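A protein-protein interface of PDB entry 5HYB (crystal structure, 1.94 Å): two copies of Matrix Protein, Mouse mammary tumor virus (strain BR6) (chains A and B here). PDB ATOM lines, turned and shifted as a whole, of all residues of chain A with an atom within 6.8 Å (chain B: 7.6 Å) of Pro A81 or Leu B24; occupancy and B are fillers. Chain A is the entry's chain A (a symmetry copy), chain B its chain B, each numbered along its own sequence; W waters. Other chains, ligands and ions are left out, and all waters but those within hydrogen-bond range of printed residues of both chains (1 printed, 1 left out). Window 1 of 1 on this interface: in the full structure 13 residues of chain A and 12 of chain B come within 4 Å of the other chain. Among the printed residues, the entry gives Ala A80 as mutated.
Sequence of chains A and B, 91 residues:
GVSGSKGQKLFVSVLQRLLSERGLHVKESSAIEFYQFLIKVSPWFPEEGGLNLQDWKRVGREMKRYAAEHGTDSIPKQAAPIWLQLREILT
The side-chain amide nitrogen (NE2) of Gln B16 lies within hydrogen-bond range of the backbone carbonyl oxygen (O) of Val B26, 3.1 Å away.
NH1 of Arg B22 lies within hydrogen-bond range of O of Leu B18 (2.9 Å).
The backbone NH of Leu B24 lies within hydrogen-bond range of the backbone carbonyl oxygen of Leu B19 (3.2 Å).
NH1 of Arg B22 lies within salt-bridge range of OE2 of Glu B21 (2.9 Å).
N of Leu A24 lies within hydrogen-bond range of O of Leu A19 (3.3 Å).
The backbone carbonyl oxygen (O) of Ser A30 lies within hydrogen-bond range of the side-chain amide nitrogen (NE2) of Gln A78, at 3.0 Å.
Water W1 lies within hydrogen-bond range of the backbone carbonyl oxygen of Gly B23 (2.5 Å), the backbone NH of Lys A27 (3.0 Å), the side-chain hydroxyl of Ser A30 (3.2 Å) and a ring nitrogen (NE2) of His B25 (3.3 Å).
Among the printed residues, pairs that only touch across the chains: Leu A84 with Glu B88 (3.2 Å), Gln A78 with Arg B22 (3.3 Å), Pro A81 with Gln B85 (3.6 Å), His A25 with Leu B24 (3.6 Å), Leu A24 with His B25 (3.7 Å), Pro A81 with Arg B22 (3.8 Å), Leu A84 with Leu B84 (3.8 Å), Leu A24 with Val B26 (3.8 Å), Val A26 with Leu B24 (3.8 Å), Lys A27 with His B25 (3.8 Å), Pro A81 with Leu B24 (3.8 Å), His A25 with Gly B23 (3.9 Å), Leu A24 with Pro B81 (3.9 Å), Lys A77 with Arg B22 (3.9 Å), Val A26 with Gly B23 (3.96 Å) and Lys A77 with Glu B21 (3.99 Å).
Hydrophobic or aromatic side chains of chain B that line the printed part of chain A: Leu B24, His B25, Val B26, Pro B81 and Leu B84.
Along chain B the printed residues that touch a printed residue of chain A span positions 21 to 88.
Among the printed residues, 19 pairs touch across the chains.
Leu A24 touches His B25, and with the chains exchanged His A25 touches Leu B24.
His A25 touches its own counterpart, His B25.
Pro A81 touches Gln B85, and with the chains exchanged Gln A85 touches Pro B81.
Gln A85 touches its own counterpart, Gln B85.
8 positions are printed for both chains.
Of the printed residues of chain B, Lys A27 touches His B25.
No residue of chain B comes within 4 Å of Ala A80.
Of chain B, only Arg B22 (3.8 Å), Leu B24 (3.8 Å) and Gln B85 (3.6 Å) come within 4 Å of Pro A81.
Printed residues of chain A within 4 Å of Gly B23: His A25 (3.9 Å) and Val A26 (3.96 Å).
Of chain A, only His A25 (3.6 Å), Val A26 (3.8 Å) and Pro A81 (3.8 Å) come within 4 Å of Leu B24.
Printed residues of chain A within 4 Å of His B25: Leu A24, His A25 and Lys A27.
Of the printed residues of chain A, Val B26 touches Leu A24.
Of the printed residues of chain A, Pro B81 touches Leu A24 and Gln A85.
The nearest printed residue of chain B that does not touch Gln A85 is Leu B84 (4.5 Å).
The backbone carbonyl oxygen (O) of His B25 is in hydrogen-bond range of the backbone NH (N) of His A25, at 2.8 Å.
The backbone carbonyl oxygen of Pro B81 lies within hydrogen-bond range of the side-chain amide nitrogen of Gln A85.
The side-chain amide nitrogen (NE2) of Gln A85 lies close to the side-chain amide nitrogen (NE2) of Gln B85, 3.5 Å away.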
ATOM      1  N   LEU A  19     -24.855  11.391  11.543  1.00  0.00           N
ATOM      2  CA  LEU A  19     -24.259  12.507  12.242  1.00  0.00           C
ATOM      3  C   LEU A  19     -23.321  12.064  13.335  1.00  0.00           C
ATOM      4  O   LEU A  19     -22.204  12.591  13.422  1.00  0.00           O
ATOM      5  CB  LEU A  19     -25.343  13.453  12.802  1.00  0.00           C
ATOM      6  CG  LEU A  19     -26.065  14.296  11.731  1.00  0.00           C
ATOM      7  CD1 LEU A  19     -27.076  15.257  12.355  1.00  0.00           C
ATOM      8  CD2 LEU A  19     -25.086  15.074  10.860  1.00  0.00           C
ATOM      9  N   LEU A  24     -21.098  14.540  15.820  1.00  0.00           N
ATOM     10  CA  LEU A  24     -22.142  15.550  16.042  1.00  0.00           C
ATOM     11  C   LEU A  24     -23.459  14.830  16.381  1.00  0.00           C
ATOM     12  O   LEU A  24     -23.850  13.837  15.741  1.00  0.00           O
ATOM     13  CB  LEU A  24     -22.323  16.472  14.827  1.00  0.00           C
ATOM     14  CG  LEU A  24     -21.217  17.505  14.441  1.00  0.00           C
ATOM     15  CD1 LEU A  24     -21.663  18.123  13.138  1.00  0.00           C
ATOM     16  CD2 LEU A  24     -20.962  18.625  15.437  1.00  0.00           C
ATOM     17  N   HIS A  25     -24.097  15.317  17.430  1.00  0.00           N
ATOM     18  CA  HIS A  25     -25.249  14.653  17.993  1.00  0.00           C
ATOM     19  C   HIS A  25     -26.381  15.601  17.939  1.00  0.00           C
ATOM     20  O   HIS A  25     -26.206  16.806  18.146  1.00  0.00           O
ATOM     21  CB  HIS A  25     -24.903  14.168  19.405  1.00  0.00           C
ATOM     22  CG  HIS A  25     -23.797  13.120  19.397  1.00  0.00           C
ATOM     23  ND1 HIS A  25     -22.506  13.410  19.731  1.00  0.00           N
ATOM     24  CD2 HIS A  25     -23.809  11.798  18.972  1.00  0.00           C
ATOM     25  CE1 HIS A  25     -21.748  12.311  19.536  1.00  0.00           C
ATOM     26  NE2 HIS A  25     -22.544  11.324  19.061  1.00  0.00           N
ATOM     27  N   VAL A  26     -27.545  15.069  17.573  1.00  0.00           N
ATOM     28  CA  VAL A  26     -28.791  15.834  17.567  1.00  0.00           C
ATOM     29  C   VAL A  26     -29.786  15.174  18.528  1.00  0.00           C
ATOM     30  O   VAL A  26     -29.915  13.929  18.560  1.00  0.00           O
ATOM     31  CB  VAL A  26     -29.389  15.898  16.138  1.00  0.00           C
ATOM     32  CG1 VAL A  26     -30.699  16.675  16.137  1.00  0.00           C
ATOM     33  CG2 VAL A  26     -28.378  16.528  15.193  1.00  0.00           C
ATOM     34  N   LYS A  27     -30.456  16.021  19.303  1.00  0.00           N
ATOM     35  CA  LYS A  27     -31.621  15.619  20.109  1.00  0.00           C
ATOM     36  C   LYS A  27     -32.708  15.013  19.233  1.00  0.00           C
ATOM     37  O   LYS A  27     -32.882  15.400  18.110  1.00  0.00           O
ATOM     38  CB  LYS A  27     -32.193  16.797  20.865  1.00  0.00           C
ATOM     39  CG  LYS A  27     -31.264  17.404  21.920  1.00  0.00           C
ATOM     40  CD  LYS A  27     -31.963  18.598  22.561  1.00  0.00           C
ATOM     41  CE  LYS A  27     -31.111  19.282  23.625  1.00  0.00           C
ATOM     42  NZ  LYS A  27     -31.992  20.095  24.531  1.00  0.00           N
ATOM     43  N   SER A  30     -35.227  17.700  18.014  1.00  0.00           N
ATOM     44  CA  SER A  30     -34.722  18.487  16.875  1.00  0.00           C
ATOM     45  C   SER A  30     -34.718  17.727  15.560  1.00  0.00           C
ATOM     46  O   SER A  30     -35.066  18.294  14.535  1.00  0.00           O
ATOM     47  CB  SER A  30     -33.292  19.003  17.171  1.00  0.00           C
ATOM     48  OG  SER A  30     -33.229  19.539  18.507  1.00  0.00           O
ATOM     49  N   PHE A  34     -36.675  18.646  12.195  1.00  0.00           N
ATOM     50  CA  PHE A  34     -35.997  18.675  10.913  1.00  0.00           C
ATOM     51  C   PHE A  34     -36.739  17.785   9.892  1.00  0.00           C
ATOM     52  O   PHE A  34     -37.003  18.203   8.738  1.00  0.00           O
ATOM     53  CB  PHE A  34     -34.513  18.268  11.072  1.00  0.00           C
ATOM     54  CG  PHE A  34     -33.748  18.302   9.797  1.00  0.00           C
ATOM     55  CD1 PHE A  34     -33.343  19.515   9.244  1.00  0.00           C
ATOM     56  CD2 PHE A  34     -33.513  17.135   9.079  1.00  0.00           C
ATOM     57  CE1 PHE A  34     -32.708  19.568   8.025  1.00  0.00           C
ATOM     58  CE2 PHE A  34     -32.848  17.193   7.849  1.00  0.00           C
ATOM     59  CZ  PHE A  34     -32.430  18.420   7.344  1.00  0.00           C
ATOM     60  N   PRO A  76     -36.743  25.884  11.208  1.00  0.00           N
ATOM     61  CA  PRO A  76     -36.034  25.505  12.419  1.00  0.00           C
ATOM     62  C   PRO A  76     -34.574  25.948  12.383  1.00  0.00           C
ATOM     63  O   PRO A  76     -33.916  25.767  11.357  1.00  0.00           O
ATOM     64  CB  PRO A  76     -36.141  23.967  12.422  1.00  0.00           C
ATOM     65  CG  PRO A  76     -37.327  23.648  11.564  1.00  0.00           C
ATOM     66  CD  PRO A  76     -37.336  24.721  10.521  1.00  0.00           C
ATOM     67  N   LYS A  77     -34.084  26.531  13.489  1.00  0.00           N
ATOM     68  CA  LYS A  77     -32.663  26.907  13.621  1.00  0.00           C
ATOM     69  C   LYS A  77     -31.673  25.743  13.329  1.00  0.00           C
ATOM     70  O   LYS A  77     -30.547  25.988  12.911  1.00  0.00           O
ATOM     71  CB  LYS A  77     -32.357  27.488  15.027  1.00  0.00           C
ATOM     72  CG  LYS A  77     -33.140  28.746  15.437  1.00  0.00           C
ATOM     73  CD  LYS A  77     -32.532  29.434  16.666  1.00  0.00           C
ATOM     74  N   GLN A  78     -32.071  24.493  13.551  1.00  0.00           N
ATOM     75  CA  GLN A  78     -31.171  23.351  13.235  1.00  0.00           C
ATOM     76  C   GLN A  78     -31.187  22.891  11.761  1.00  0.00           C
ATOM     77  O   GLN A  78     -30.371  22.034  11.326  1.00  0.00           O
ATOM     78  CB  GLN A  78     -31.463  22.165  14.159  1.00  0.00           C
ATOM     79  CG  GLN A  78     -32.794  21.454  13.900  1.00  0.00           C
ATOM     80  CD  GLN A  78     -33.965  22.057  14.665  1.00  0.00           C
ATOM     81  OE1 GLN A  78     -33.924  23.206  15.078  1.00  0.00           O
ATOM     82  NE2 GLN A  78     -35.008  21.262  14.872  1.00  0.00           N
ATOM     83  N   ALA A  79     -32.108  23.455  10.988  1.00  0.00           N
ATOM     84  CA  ALA A  79     -32.292  23.056   9.607  1.00  0.00           C
ATOM     85  C   ALA A  79     -31.023  23.243   8.768  1.00  0.00           C
ATOM     86  O   ALA A  79     -30.547  22.288   8.153  1.00  0.00           O
ATOM     87  CB  ALA A  79     -33.480  23.783   8.991  1.00  0.00           C
ATOM     88  N   ALA A  80     -30.437  24.435   8.791  1.00  0.00           N
ATOM     89  CA  ALA A  80     -29.282  24.706   7.927  1.00  0.00           C
ATOM     90  C   ALA A  80     -28.042  23.911   8.389  1.00  0.00           C
ATOM     91  O   ALA A  80     -27.321  23.305   7.587  1.00  0.00           O
ATOM     92  CB  ALA A  80     -29.014  26.218   7.803  1.00  0.00           C
ATOM     93  N   PRO A  81     -27.812  23.855   9.694  1.00  0.00           N
ATOM     94  CA  PRO A  81     -26.680  23.106  10.247  1.00  0.00           C
ATOM     95  C   PRO A  81     -26.667  21.598   9.934  1.00  0.00           C
ATOM     96  O   PRO A  81     -25.644  21.032   9.457  1.00  0.00           O
ATOM     97  CB  PRO A  81     -26.803  23.392  11.743  1.00  0.00           C
ATOM     98  CG  PRO A  81     -27.441  24.728  11.798  1.00  0.00           C
ATOM     99  CD  PRO A  81     -28.428  24.728  10.700  1.00  0.00           C
ATOM    100  N   ILE A  82     -27.822  20.961  10.147  1.00  0.00           N
ATOM    101  CA  ILE A  82     -28.028  19.570   9.784  1.00  0.00           C
ATOM    102  C   ILE A  82     -27.890  19.333   8.295  1.00  0.00           C
ATOM    103  O   ILE A  82     -27.234  18.381   7.861  1.00  0.00           O
ATOM    104  CB  ILE A  82     -29.430  19.047  10.216  1.00  0.00           C
ATOM    105  CG1 ILE A  82     -29.537  19.076  11.735  1.00  0.00           C
ATOM    106  CG2 ILE A  82     -29.629  17.608   9.668  1.00  0.00           C
ATOM    107  CD1 ILE A  82     -30.926  18.783  12.305  1.00  0.00           C
ATOM    108  N   TRP A  83     -28.536  20.177   7.500  1.00  0.00           N
ATOM    109  CA  TRP A  83     -28.387  20.044   6.061  1.00  0.00           C
ATOM    110  C   TRP A  83     -26.943  20.120   5.606  1.00  0.00           C
ATOM    111  O   TRP A  83     -26.495  19.439   4.670  1.00  0.00           O
ATOM    112  CB  TRP A  83     -29.177  21.132   5.349  1.00  0.00           C
ATOM    113  CG  TRP A  83     -29.057  20.990   3.846  1.00  0.00           C
ATOM    114  CD1 TRP A  83     -29.848  20.251   2.995  1.00  0.00           C
ATOM    115  CD2 TRP A  83     -28.017  21.557   3.006  1.00  0.00           C
ATOM    116  NE1 TRP A  83     -29.393  20.343   1.692  1.00  0.00           N
ATOM    117  CE2 TRP A  83     -28.306  21.118   1.634  1.00  0.00           C
ATOM    118  CE3 TRP A  83     -26.928  22.399   3.238  1.00  0.00           C
ATOM    119  CZ2 TRP A  83     -27.524  21.506   0.561  1.00  0.00           C
ATOM    120  CZ3 TRP A  83     -26.128  22.777   2.154  1.00  0.00           C
ATOM    121  CH2 TRP A  83     -26.427  22.344   0.839  1.00  0.00           C
ATOM    122  N   LEU A  84     -26.195  20.988   6.246  1.00  0.00           N
ATOM    123  CA  LEU A  84     -24.805  21.231   5.834  1.00  0.00           C
ATOM    124  C   LEU A  84     -23.918  20.044   6.192  1.00  0.00           C
ATOM    125  O   LEU A  84     -23.056  19.649   5.404  1.00  0.00           O
ATOM    126  CB  LEU A  84     -24.318  22.498   6.543  1.00  0.00           C
ATOM    127  CG  LEU A  84     -22.896  22.974   6.335  1.00  0.00           C
ATOM    128  CD1 LEU A  84     -22.648  23.453   4.886  1.00  0.00           C
ATOM    129  CD2 LEU A  84     -22.670  24.086   7.362  1.00  0.00           C
ATOM    130  N   GLN A  85     -24.092  19.504   7.395  1.00  0.00           N
ATOM    131  CA  GLN A  85     -23.345  18.306   7.790  1.00  0.00           C
ATOM    132  C   GLN A  85     -23.632  17.164   6.868  1.00  0.00           C
ATOM    133  O   GLN A  85     -22.730  16.483   6.487  1.00  0.00           O
ATOM    134  CB  GLN A  85     -23.647  17.886   9.222  1.00  0.00           C
ATOM    135  CG  GLN A  85     -23.107  18.874  10.272  1.00  0.00           C
ATOM    136  CD  GLN A  85     -21.618  19.257  10.096  1.00  0.00           C
ATOM    137  OE1 GLN A  85     -20.799  18.411   9.726  1.00  0.00           O
ATOM    138  NE2 GLN A  85     -21.266  20.551  10.373  1.00  0.00           N
ATOM    139  N   LEU A  86     -24.898  16.935   6.505  1.00  0.00           N
ATOM    140  CA  LEU A  86     -25.239  15.848   5.586  1.00  0.00           C
ATOM    141  C   LEU A  86     -24.648  16.099   4.209  1.00  0.00           C
ATOM    142  O   LEU A  86     -24.254  15.173   3.497  1.00  0.00           O
ATOM    143  CB  LEU A  86     -26.765  15.662   5.494  1.00  0.00           C
ATOM    144  CG  LEU A  86     -27.373  14.844   6.642  1.00  0.00           C
ATOM    145  CD1 LEU A  86     -28.883  15.051   6.764  1.00  0.00           C
ATOM    146  CD2 LEU A  86     -27.036  13.368   6.445  1.00  0.00           C
ATOM    147  N   LEU B  15     -17.602  26.635  22.611  1.00  0.00           N
ATOM    148  CA  LEU B  15     -17.980  25.799  21.485  1.00  0.00           C
ATOM    149  C   LEU B  15     -19.354  25.206  21.761  1.00  0.00           C
ATOM    150  O   LEU B  15     -20.239  25.220  20.889  1.00  0.00           O
ATOM    151  CB  LEU B  15     -16.982  24.682  21.246  1.00  0.00           C
ATOM    152  CG  LEU B  15     -17.305  23.764  20.044  1.00  0.00           C
ATOM    153  CD1 LEU B  15     -17.178  24.532  18.714  1.00  0.00           C
ATOM    154  CD2 LEU B  15     -16.387  22.563  20.059  1.00  0.00           C
ATOM    155  N   GLN B  16     -19.548  24.716  22.973  1.00  0.00           N
ATOM    156  CA  GLN B  16     -20.782  24.037  23.294  1.00  0.00           C
ATOM    157  C   GLN B  16     -22.005  24.988  23.299  1.00  0.00           C
ATOM    158  O   GLN B  16     -23.095  24.571  22.933  1.00  0.00           O
ATOM    159  CB  GLN B  16     -20.622  23.181  24.575  1.00  0.00           C
ATOM    160  CG  GLN B  16     -19.651  21.978  24.391  1.00  0.00           C
ATOM    161  CD  GLN B  16     -19.662  20.959  25.543  1.00  0.00           C
ATOM    162  OE1 GLN B  16     -20.022  21.281  26.699  1.00  0.00           O
ATOM    163  NE2 GLN B  16     -19.243  19.713  25.234  1.00  0.00           N
ATOM    164  N   ARG B  17     -21.831  26.252  23.669  1.00  0.00           N
ATOM    165  CA  ARG B  17     -22.913  27.221  23.601  1.00  0.00           C
ATOM    166  C   ARG B  17     -23.255  27.567  22.137  1.00  0.00           C
ATOM    167  O   ARG B  17     -24.428  27.633  21.757  1.00  0.00           O
ATOM    168  CB  ARG B  17     -22.517  28.488  24.348  1.00  0.00           C
ATOM    169  CG  ARG B  17     -23.543  29.602  24.268  1.00  0.00           C
ATOM    170  CD  ARG B  17     -23.162  30.740  25.200  1.00  0.00           C
ATOM    171  NE  ARG B  17     -23.407  30.285  26.555  1.00  0.00           N
ATOM    172  CZ  ARG B  17     -24.532  30.493  27.235  1.00  0.00           C
ATOM    173  NH1 ARG B  17     -25.520  31.239  26.726  1.00  0.00           N
ATOM    174  NH2 ARG B  17     -24.662  29.953  28.443  1.00  0.00           N
ATOM    175  N   LEU B  18     -22.228  27.779  21.322  1.00  0.00           N
ATOM    176  CA  LEU B  18     -22.456  28.206  19.939  1.00  0.00           C
ATOM    177  C   LEU B  18     -23.109  27.091  19.126  1.00  0.00           C
ATOM    178  O   LEU B  18     -24.001  27.351  18.333  1.00  0.00           O
ATOM    179  CB  LEU B  18     -21.142  28.625  19.293  1.00  0.00           C
ATOM    180  CG  LEU B  18     -20.442  29.840  19.900  1.00  0.00           C
ATOM    181  CD1 LEU B  18     -19.084  30.053  19.210  1.00  0.00           C
ATOM    182  CD2 LEU B  18     -21.317  31.087  19.815  1.00  0.00           C
ATOM    183  N   LEU B  19     -22.667  25.862  19.343  1.00  0.00           N
ATOM    184  CA  LEU B  19     -23.185  24.739  18.597  1.00  0.00           C
ATOM    185  C   LEU B  19     -24.594  24.383  19.101  1.00  0.00           C
ATOM    186  O   LEU B  19     -25.512  24.234  18.292  1.00  0.00           O
ATOM    187  CB  LEU B  19     -22.226  23.563  18.667  1.00  0.00           C
ATOM    188  CG  LEU B  19     -20.965  23.673  17.797  1.00  0.00           C
ATOM    189  CD1 LEU B  19     -20.150  22.405  18.037  1.00  0.00           C
ATOM    190  CD2 LEU B  19     -21.297  23.817  16.315  1.00  0.00           C
ATOM    191  N   SER B  20     -24.784  24.343  20.421  1.00  0.00           N
ATOM    192  CA  SER B  20     -26.088  23.981  20.984  1.00  0.00           C
ATOM    193  C   SER B  20     -27.196  24.931  20.550  1.00  0.00           C
ATOM    194  O   SER B  20     -28.350  24.514  20.395  1.00  0.00           O
ATOM    195  CB  SER B  20     -26.058  23.850  22.522  1.00  0.00           C
ATOM    196  OG  SER B  20     -25.984  25.117  23.149  1.00  0.00           O
ATOM    197  N   GLU B  21     -26.887  26.198  20.294  1.00  0.00           N
ATOM    198  CA  GLU B  21     -27.973  27.067  19.827  1.00  0.00           C
ATOM    199  C   GLU B  21     -28.338  26.848  18.353  1.00  0.00           C
ATOM    200  O   GLU B  21     -29.327  27.391  17.871  1.00  0.00           O
ATOM    201  CB  GLU B  21     -27.765  28.542  20.192  1.00  0.00           C
ATOM    202  CG  GLU B  21     -26.639  29.274  19.494  1.00  0.00           C
ATOM    203  CD  GLU B  21     -26.219  30.576  20.215  1.00  0.00           C
ATOM    204  OE1 GLU B  21     -26.915  31.003  21.169  1.00  0.00           O
ATOM    205  OE2 GLU B  21     -25.180  31.184  19.845  1.00  0.00           O
ATOM    206  N   ARG B  22     -27.592  26.001  17.659  1.00  0.00           N
ATOM    207  CA  ARG B  22     -27.954  25.569  16.301  1.00  0.00           C
ATOM    208  C   ARG B  22     -28.426  24.108  16.275  1.00  0.00           C
ATOM    209  O   ARG B  22     -28.542  23.495  15.197  1.00  0.00           O
ATOM    210  CB  ARG B  22     -26.753  25.680  15.380  1.00  0.00           C
ATOM    211  CG  ARG B  22     -26.553  27.043  14.775  1.00  0.00           C
ATOM    212  CD  ARG B  22     -25.487  27.816  15.511  1.00  0.00           C
ATOM    213  NE  ARG B  22     -25.656  29.256  15.227  1.00  0.00           N
ATOM    214  CZ  ARG B  22     -25.286  30.241  16.039  1.00  0.00           C
ATOM    215  NH1 ARG B  22     -24.685  29.990  17.231  1.00  0.00           N
ATOM    216  NH2 ARG B  22     -25.528  31.492  15.653  1.00  0.00           N
ATOM    217  N   GLY B  23     -28.620  23.535  17.468  1.00  0.00           N
ATOM    218  CA  GLY B  23     -29.114  22.144  17.604  1.00  0.00           C
ATOM    219  C   GLY B  23     -28.073  21.028  17.524  1.00  0.00           C
ATOM    220  O   GLY B  23     -28.448  19.850  17.350  1.00  0.00           O
ATOM    221  N   LEU B  24     -26.783  21.357  17.610  1.00  0.00           N
ATOM    222  CA  LEU B  24     -25.723  20.328  17.486  1.00  0.00           C
ATOM    223  C   LEU B  24     -24.891  20.199  18.776  1.00  0.00           C
ATOM    224  O   LEU B  24     -24.662  21.177  19.497  1.00  0.00           O
ATOM    225  CB  LEU B  24     -24.795  20.588  16.298  1.00  0.00           C
ATOM    226  CG  LEU B  24     -25.425  20.674  14.905  1.00  0.00           C
ATOM    227  CD1 LEU B  24     -24.446  21.310  13.927  1.00  0.00           C
ATOM    228  CD2 LEU B  24     -25.902  19.312  14.402  1.00  0.00           C
ATOM    229  N   HIS B  25     -24.476  18.977  19.076  1.00  0.00           N
ATOM    230  CA  HIS B  25     -23.924  18.669  20.382  1.00  0.00           C
ATOM    231  C   HIS B  25     -22.768  17.775  20.175  1.00  0.00           C
ATOM    232  O   HIS B  25     -22.861  16.801  19.424  1.00  0.00           O
ATOM    233  CB  HIS B  25     -24.970  18.016  21.290  1.00  0.00           C
ATOM    234  CG  HIS B  25     -26.175  18.884  21.526  1.00  0.00           C
ATOM    235  ND1 HIS B  25     -26.290  19.669  22.581  1.00  0.00           N
ATOM    236  CD2 HIS B  25     -27.334  19.078  20.765  1.00  0.00           C
ATOM    237  CE1 HIS B  25     -27.458  20.349  22.533  1.00  0.00           C
ATOM    238  NE2 HIS B  25     -28.091  19.999  21.416  1.00  0.00           N
ATOM    239  N   VAL B  26     -21.648  18.154  20.805  1.00  0.00           N
ATOM    240  CA  VAL B  26     -20.379  17.442  20.690  1.00  0.00           C
ATOM    241  C   VAL B  26     -20.055  16.924  22.091  1.00  0.00           C
ATOM    242  O   VAL B  26     -20.132  17.676  23.061  1.00  0.00           O
ATOM    243  CB  VAL B  26     -19.213  18.395  20.239  1.00  0.00           C
ATOM    244  CG1 VAL B  26     -17.943  17.599  20.064  1.00  0.00           C
ATOM    245  CG2 VAL B  26     -19.561  19.137  18.938  1.00  0.00           C
ATOM    246  N   PRO B  81     -16.230  18.805  10.370  1.00  0.00           N
ATOM    247  CA  PRO B  81     -17.609  19.198  10.780  1.00  0.00           C
ATOM    248  C   PRO B  81     -17.685  20.423  11.703  1.00  0.00           C
ATOM    249  O   PRO B  81     -18.472  21.337  11.448  1.00  0.00           O
ATOM    250  CB  PRO B  81     -18.093  17.963  11.535  1.00  0.00           C
ATOM    251  CG  PRO B  81     -17.420  16.841  10.839  1.00  0.00           C
ATOM    252  CD  PRO B  81     -16.036  17.348  10.449  1.00  0.00           C
ATOM    253  N   ILE B  82     -16.896  20.427  12.779  1.00  0.00           N
ATOM    254  CA  ILE B  82     -16.881  21.550  13.730  1.00  0.00           C
ATOM    255  C   ILE B  82     -16.382  22.842  13.022  1.00  0.00           C
ATOM    256  O   ILE B  82     -16.990  23.923  13.159  1.00  0.00           O
ATOM    257  CB  ILE B  82     -16.057  21.223  15.027  1.00  0.00           C
ATOM    258  CG1 ILE B  82     -16.734  20.126  15.881  1.00  0.00           C
ATOM    259  CG2 ILE B  82     -15.881  22.469  15.890  1.00  0.00           C
ATOM    260  CD1 ILE B  82     -15.836  19.418  16.889  1.00  0.00           C
ATOM    261  N   LEU B  84     -16.530  23.587   9.978  1.00  0.00           N
ATOM    262  CA  LEU B  84     -17.529  24.004   9.007  1.00  0.00           C
ATOM    263  C   LEU B  84     -18.676  24.714   9.690  1.00  0.00           C
ATOM    264  O   LEU B  84     -19.121  25.746   9.227  1.00  0.00           O
ATOM    265  CB  LEU B  84     -18.036  22.803   8.233  1.00  0.00           C
ATOM    266  CG  LEU B  84     -19.009  23.115   7.101  1.00  0.00           C
ATOM    267  CD1 LEU B  84     -18.567  24.323   6.273  1.00  0.00           C
ATOM    268  CD2 LEU B  84     -19.103  21.879   6.219  1.00  0.00           C
ATOM    269  N   GLN B  85     -19.138  24.157  10.814  1.00  0.00           N
ATOM    270  CA  GLN B  85     -20.238  24.763  11.543  1.00  0.00           C
ATOM    271  C   GLN B  85     -19.908  26.150  12.117  1.00  0.00           C
ATOM    272  O   GLN B  85     -20.747  27.096  12.057  1.00  0.00           O
ATOM    273  CB  GLN B  85     -20.708  23.829  12.648  1.00  0.00           C
ATOM    274  CG  GLN B  85     -22.028  24.286  13.210  1.00  0.00           C
ATOM    275  CD  GLN B  85     -23.125  24.333  12.142  1.00  0.00           C
ATOM    276  OE1 GLN B  85     -23.802  25.380  11.958  1.00  0.00           O
ATOM    277  NE2 GLN B  85     -23.271  23.216  11.399  1.00  0.00           N
ATOM    278  N   GLU B  88     -20.009  28.719   9.381  1.00  0.00           N
ATOM    279  CA  GLU B  88     -21.374  29.147   9.082  1.00  0.00           C
ATOM    280  C   GLU B  88     -21.888  30.064  10.141  1.00  0.00           C
ATOM    281  O   GLU B  88     -22.481  31.065   9.825  1.00  0.00           O
ATOM    282  CB  GLU B  88     -22.319  27.964   8.913  1.00  0.00           C
ATOM    283  CG  GLU B  88     -22.039  27.192   7.648  1.00  0.00           C
ATOM    284  CD  GLU B  88     -22.113  28.045   6.381  1.00  0.00           C
ATOM    285  OE1 GLU B  88     -23.205  28.600   6.109  1.00  0.00           O
ATOM    286  OE2 GLU B  88     -21.072  28.156   5.681  1.00  0.00           O
ATOM    287  N   ILE B  89     -21.638  29.741  11.405  1.00  0.00           N
ATOM    288  CA  ILE B  89     -22.038  30.620  12.495  1.00  0.00           C
ATOM    289  C   ILE B  89     -21.444  32.016  12.279  1.00  0.00           C
ATOM    290  O   ILE B  89     -22.116  33.002  12.494  1.00  0.00           O
ATOM    291  CB  ILE B  89     -21.639  30.041  13.866  1.00  0.00           C
ATOM    292  CG1 ILE B  89     -22.492  28.813  14.170  1.00  0.00           C
ATOM    293  CG2 ILE B  89     -21.816  31.063  14.984  1.00  0.00           C
ATOM    294  CD1 ILE B  89     -21.851  27.872  15.177  1.00  0.00           C
HETATM  295  O   HOH W   1     -30.135  19.030  18.981  1.00  0.00           O
